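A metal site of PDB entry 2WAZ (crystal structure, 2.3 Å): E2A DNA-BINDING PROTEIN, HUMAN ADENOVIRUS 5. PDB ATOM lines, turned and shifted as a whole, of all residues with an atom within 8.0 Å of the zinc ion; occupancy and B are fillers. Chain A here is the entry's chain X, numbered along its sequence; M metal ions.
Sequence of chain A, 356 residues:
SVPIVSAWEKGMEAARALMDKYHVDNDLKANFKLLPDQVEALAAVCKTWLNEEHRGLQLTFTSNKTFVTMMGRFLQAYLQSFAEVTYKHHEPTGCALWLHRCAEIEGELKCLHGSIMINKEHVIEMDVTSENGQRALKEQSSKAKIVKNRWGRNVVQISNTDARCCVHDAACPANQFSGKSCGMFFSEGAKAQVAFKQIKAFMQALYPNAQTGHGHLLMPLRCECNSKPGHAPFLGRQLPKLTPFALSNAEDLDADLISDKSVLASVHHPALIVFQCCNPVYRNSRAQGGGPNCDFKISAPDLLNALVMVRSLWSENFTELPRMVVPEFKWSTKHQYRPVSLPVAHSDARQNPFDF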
ATOM      1  N   LYS A 110      12.851 -19.889  16.026  1.00  0.00           N
ATOM      2  CA  LYS A 110      12.491 -20.994  16.943  1.00  0.00           C
ATOM      3  C   LYS A 110      11.051 -21.477  16.704  1.00  0.00           C
ATOM      4  O   LYS A 110      10.197 -20.646  16.394  1.00  0.00           O
ATOM      5  CB  LYS A 110      12.673 -20.584  18.387  1.00  0.00           C
ATOM      6  CG  LYS A 110      14.116 -20.315  18.685  1.00  0.00           C
ATOM      7  CD  LYS A 110      14.294 -19.657  20.015  1.00  0.00           C
ATOM      8  CE  LYS A 110      15.754 -19.140  20.181  1.00  0.00           C
ATOM      9  NZ  LYS A 110      16.122 -17.769  19.456  1.00  0.00           N
ATOM     10  N   CYS A 111      10.778 -22.778  16.888  1.00  0.00           N
ATOM     11  CA  CYS A 111       9.458 -23.299  16.593  1.00  0.00           C
ATOM     12  C   CYS A 111       8.683 -23.328  17.893  1.00  0.00           C
ATOM     13  O   CYS A 111       9.180 -22.839  18.901  1.00  0.00           O
ATOM     14  CB  CYS A 111       9.505 -24.706  15.981  1.00  0.00           C
ATOM     15  SG  CYS A 111      10.198 -25.900  17.112  1.00  0.00           S
ATOM     16  N   LEU A 112       7.496 -23.926  17.872  1.00  0.00           N
ATOM     17  CA  LEU A 112       6.609 -23.937  19.041  1.00  0.00           C
ATOM     18  C   LEU A 112       7.192 -24.711  20.206  1.00  0.00           C
ATOM     19  O   LEU A 112       6.767 -24.528  21.358  1.00  0.00           O
ATOM     20  CB  LEU A 112       5.217 -24.520  18.684  1.00  0.00           C
ATOM     21  CG  LEU A 112       4.067 -23.687  18.063  1.00  0.00           C
ATOM     22  CD1 LEU A 112       4.187 -22.112  17.982  1.00  0.00           C
ATOM     23  CD2 LEU A 112       3.435 -24.355  16.802  1.00  0.00           C
ATOM     24  N   HIS A 113       8.149 -25.583  19.921  1.00  0.00           N
ATOM     25  CA  HIS A 113       8.860 -26.269  20.996  1.00  0.00           C
ATOM     26  C   HIS A 113       9.749 -25.333  21.754  1.00  0.00           C
ATOM     27  O   HIS A 113      10.244 -25.720  22.827  1.00  0.00           O
ATOM     28  CB  HIS A 113       9.737 -27.413  20.489  1.00  0.00           C
ATOM     29  CG  HIS A 113       8.961 -28.576  19.938  1.00  0.00           C
ATOM     30  ND1 HIS A 113       8.556 -28.639  18.614  1.00  0.00           N
ATOM     31  CD2 HIS A 113       8.516 -29.706  20.541  1.00  0.00           C
ATOM     32  CE1 HIS A 113       7.906 -29.776  18.427  1.00  0.00           C
ATOM     33  NE2 HIS A 113       7.840 -30.433  19.585  1.00  0.00           N
ATOM     34  N   GLY A 114      10.001 -24.142  21.187  1.00  0.00           N
ATOM     35  CA  GLY A 114      10.972 -23.196  21.760  1.00  0.00           C
ATOM     36  C   GLY A 114      12.453 -23.516  21.442  1.00  0.00           C
ATOM     37  O   GLY A 114      13.357 -22.852  21.947  1.00  0.00           O
ATOM     38  N   SER A 115      12.690 -24.506  20.572  1.00  0.00           N
ATOM     39  CA  SER A 115      14.063 -24.821  20.140  1.00  0.00           C
ATOM     40  C   SER A 115      14.331 -24.274  18.739  1.00  0.00           C
ATOM     41  O   SER A 115      13.368 -24.068  17.935  1.00  0.00           O
ATOM     42  CB  SER A 115      14.324 -26.329  20.165  1.00  0.00           C
ATOM     43  OG  SER A 115      13.287 -27.005  19.473  1.00  0.00           O
ATOM     44  N   ILE A 116      15.608 -24.033  18.432  1.00  0.00           N
ATOM     45  CA  ILE A 116      15.933 -23.470  17.183  1.00  0.00           C
ATOM     46  C   ILE A 116      15.459 -24.369  15.997  1.00  0.00           C
ATOM     47  O   ILE A 116      15.439 -25.605  16.118  1.00  0.00           O
ATOM     48  CB  ILE A 116      17.471 -22.956  17.005  1.00  0.00           C
ATOM     49  CG1 ILE A 116      18.259 -23.879  16.200  1.00  0.00           C
ATOM     50  CG2 ILE A 116      18.270 -22.484  18.309  1.00  0.00           C
ATOM     51  CD1 ILE A 116      19.015 -23.102  15.169  1.00  0.00           C
ATOM     52  N   MET A 117      15.098 -23.737  14.873  1.00  0.00           N
ATOM     53  CA  MET A 117      14.773 -24.430  13.642  1.00  0.00           C
ATOM     54  C   MET A 117      16.017 -24.734  12.747  1.00  0.00           C
ATOM     55  O   MET A 117      16.924 -23.889  12.595  1.00  0.00           O
ATOM     56  CB  MET A 117      13.618 -23.728  12.876  1.00  0.00           C
ATOM     57  CG  MET A 117      12.305 -23.557  13.756  1.00  0.00           C
ATOM     58  SD  MET A 117      11.042 -22.643  12.853  1.00  0.00           S
ATOM     59  CE  MET A 117      10.441 -23.984  11.759  1.00  0.00           C
ATOM     60  N   CYS A 165      12.967 -26.062   9.517  1.00  0.00           N
ATOM     61  CA  CYS A 165      12.060 -27.059   9.963  1.00  0.00           C
ATOM     62  C   CYS A 165      12.144 -27.171  11.500  1.00  0.00           C
ATOM     63  O   CYS A 165      13.151 -26.849  12.082  1.00  0.00           O
ATOM     64  CB  CYS A 165      12.388 -28.386   9.220  1.00  0.00           C
ATOM     65  SG  CYS A 165      13.880 -29.253   9.848  1.00  0.00           S
ATOM     66  N   CYS A 166      11.095 -27.632  12.146  1.00  0.00           N
ATOM     67  CA  CYS A 166      11.157 -28.178  13.486  1.00  0.00           C
ATOM     68  C   CYS A 166      12.294 -29.202  13.638  1.00  0.00           C
ATOM     69  O   CYS A 166      12.478 -30.044  12.782  1.00  0.00           O
ATOM     70  CB  CYS A 166       9.853 -28.902  13.807  1.00  0.00           C
ATOM     71  SG  CYS A 166       9.684 -29.462  15.474  1.00  0.00           S
ATOM     72  N   VAL A 167      13.042 -29.143  14.712  1.00  0.00           N
ATOM     73  CA  VAL A 167      14.208 -30.040  14.842  1.00  0.00           C
ATOM     74  C   VAL A 167      13.752 -31.535  14.804  1.00  0.00           C
ATOM     75  O   VAL A 167      14.490 -32.417  14.385  1.00  0.00           O
ATOM     76  CB  VAL A 167      15.046 -29.706  16.138  1.00  0.00           C
ATOM     77  CG1 VAL A 167      14.315 -30.147  17.403  1.00  0.00           C
ATOM     78  CG2 VAL A 167      16.453 -30.327  16.093  1.00  0.00           C
ATOM     79  N   HIS A 168      12.509 -31.783  15.226  1.00  0.00           N
ATOM     80  CA  HIS A 168      11.970 -33.139  15.210  1.00  0.00           C
ATOM     81  C   HIS A 168      11.734 -33.664  13.812  1.00  0.00           C
ATOM     82  O   HIS A 168      11.571 -34.853  13.626  1.00  0.00           O
ATOM     83  CB  HIS A 168      10.744 -33.236  16.085  1.00  0.00           C
ATOM     84  CG  HIS A 168      11.022 -32.856  17.510  1.00  0.00           C
ATOM     85  ND1 HIS A 168      11.464 -33.766  18.447  1.00  0.00           N
ATOM     86  CD2 HIS A 168      10.957 -31.663  18.146  1.00  0.00           C
ATOM     87  CE1 HIS A 168      11.610 -33.166  19.612  1.00  0.00           C
ATOM     88  NE2 HIS A 168      11.307 -31.890  19.452  1.00  0.00           N
ATOM     89  N   ASP A 169      11.786 -32.766  12.831  1.00  0.00           N
ATOM     90  CA  ASP A 169      11.607 -33.096  11.411  1.00  0.00           C
ATOM     91  C   ASP A 169      12.893 -33.049  10.639  1.00  0.00           C
ATOM     92  O   ASP A 169      12.877 -33.071   9.377  1.00  0.00           O
ATOM     93  CB  ASP A 169      10.604 -32.082  10.798  1.00  0.00           C
ATOM     94  CG  ASP A 169       9.212 -32.189  11.437  1.00  0.00           C
ATOM     95  OD1 ASP A 169       8.851 -33.310  11.908  1.00  0.00           O
ATOM     96  OD2 ASP A 169       8.485 -31.153  11.478  1.00  0.00           O
ATOM     97  N   LYS A 180       6.368 -36.153  15.976  1.00  0.00           N
ATOM     98  CA  LYS A 180       6.793 -35.263  17.073  1.00  0.00           C
ATOM     99  C   LYS A 180       6.853 -33.813  16.663  1.00  0.00           C
ATOM    100  O   LYS A 180       7.185 -32.927  17.479  1.00  0.00           O
ATOM    101  CB  LYS A 180       8.134 -35.717  17.699  1.00  0.00           C
ATOM    102  CG  LYS A 180       7.990 -36.974  18.584  1.00  0.00           C
ATOM    103  CD  LYS A 180       9.194 -37.172  19.527  1.00  0.00           C
ATOM    104  CE  LYS A 180       9.323 -38.646  19.961  1.00  0.00           C
ATOM    105  NZ  LYS A 180       7.950 -39.235  20.201  1.00  0.00           N
ATOM    106  N   SER A 181       6.543 -33.552  15.404  1.00  0.00           N
ATOM    107  CA  SER A 181       6.553 -32.195  14.871  1.00  0.00           C
ATOM    108  C   SER A 181       5.555 -31.246  15.563  1.00  0.00           C
ATOM    109  O   SER A 181       4.496 -31.678  16.014  1.00  0.00           O
ATOM    110  CB  SER A 181       6.304 -32.212  13.359  1.00  0.00           C
ATOM    111  OG  SER A 181       6.515 -30.912  12.843  1.00  0.00           O
ATOM    112  N   CYS A 182       5.907 -29.963  15.675  1.00  0.00           N
ATOM    113  CA  CYS A 182       4.945 -28.935  16.117  1.00  0.00           C
ATOM    114  C   CYS A 182       4.157 -28.385  14.920  1.00  0.00           C
ATOM    115  O   CYS A 182       3.225 -27.581  15.104  1.00  0.00           O
ATOM    116  CB  CYS A 182       5.655 -27.769  16.840  1.00  0.00           C
ATOM    117  SG  CYS A 182       6.880 -26.936  15.812  1.00  0.00           S
ATOM    118  N   GLY A 183       4.570 -28.768  13.711  1.00  0.00           N
ATOM    119  CA  GLY A 183       3.900 -28.453  12.479  1.00  0.00           C
ATOM    120  C   GLY A 183       4.421 -27.240  11.737  1.00  0.00           C
ATOM    121  O   GLY A 183       3.853 -26.828  10.731  1.00  0.00           O
ATOM    122  N   MET A 184       5.513 -26.682  12.234  1.00  0.00           N
ATOM    123  CA  MET A 184       5.979 -25.407  11.742  1.00  0.00           C
ATOM    124  C   MET A 184       7.093 -25.674  10.750  1.00  0.00           C
ATOM    125  O   MET A 184       7.984 -26.491  11.006  1.00  0.00           O
ATOM    126  CB  MET A 184       6.437 -24.553  12.942  1.00  0.00           C
ATOM    127  CG  MET A 184       6.331 -23.085  12.718  1.00  0.00           C
ATOM    128  SD  MET A 184       6.571 -22.045  14.195  1.00  0.00           S
ATOM    129  CE  MET A 184       5.453 -22.796  15.272  1.00  0.00           C
ATOM    130  N   PHE A 185       7.009 -24.983   9.611  1.00  0.00           N
ATOM    131  CA  PHE A 185       8.018 -25.047   8.594  1.00  0.00           C
ATOM    132  C   PHE A 185       7.944 -23.747   7.834  1.00  0.00           C
ATOM    133  O   PHE A 185       6.834 -23.205   7.574  1.00  0.00           O
ATOM    134  CB  PHE A 185       7.684 -26.190   7.658  1.00  0.00           C
ATOM    135  CG  PHE A 185       8.532 -26.246   6.443  1.00  0.00           C
ATOM    136  CD1 PHE A 185       9.807 -26.828   6.494  1.00  0.00           C
ATOM    137  CD2 PHE A 185       8.062 -25.753   5.248  1.00  0.00           C
ATOM    138  CE1 PHE A 185      10.628 -26.899   5.378  1.00  0.00           C
ATOM    139  CE2 PHE A 185       8.890 -25.813   4.096  1.00  0.00           C
ATOM    140  CZ  PHE A 185      10.162 -26.388   4.166  1.00  0.00           C
ATOM    141  N   TRP A 331       4.257 -25.504  25.022  1.00  0.00           N
ATOM    142  CA  TRP A 331       4.332 -26.693  24.225  1.00  0.00           C
ATOM    143  C   TRP A 331       3.784 -27.893  25.022  1.00  0.00           C
ATOM    144  O   TRP A 331       4.113 -28.058  26.194  1.00  0.00           O
ATOM    145  CB  TRP A 331       5.740 -27.015  23.746  1.00  0.00           C
ATOM    146  CG  TRP A 331       5.638 -28.330  22.992  1.00  0.00           C
ATOM    147  CD1 TRP A 331       6.049 -29.557  23.418  1.00  0.00           C
ATOM    148  CD2 TRP A 331       4.955 -28.536  21.757  1.00  0.00           C
ATOM    149  NE1 TRP A 331       5.703 -30.519  22.489  1.00  0.00           N
ATOM    150  CE2 TRP A 331       5.022 -29.917  21.460  1.00  0.00           C
ATOM    151  CE3 TRP A 331       4.308 -27.679  20.843  1.00  0.00           C
ATOM    152  CZ2 TRP A 331       4.480 -30.452  20.301  1.00  0.00           C
ATOM    153  CZ3 TRP A 331       3.778 -28.219  19.688  1.00  0.00           C
ATOM    154  CH2 TRP A 331       3.852 -29.588  19.442  1.00  0.00           C
HETATM  155 ZN    ZN M   1       8.825 -27.766  16.791  1.00  0.00          ZN
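The nearest printed residue that does not touch the zinc ion is Leu 112 (4.2 Å).
NE2 of His 113 lies within hydrogen-bond range of O of Lys 180 (3.3 Å). N of His 168 lies close to SG of Cys 166. SG of Cys 182 sits close to N of Leu 112 (3.7 Å). The side-chain sulfur (SG) of Cys 111 lies close to the backbone carbonyl oxygen (O) of Ser 115 (3.8 Å).
ND1 of His 113 is bound to the zinc ion, at 2.0 Å. SG of Cys 166 binds the zinc ion, at 2.3 Å. The side-chain sulfur (SG) of Cys 182 is bound to the zinc ion (2.3 Å). SG of Cys 111 is bound to the zinc ion (2.3 Å).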
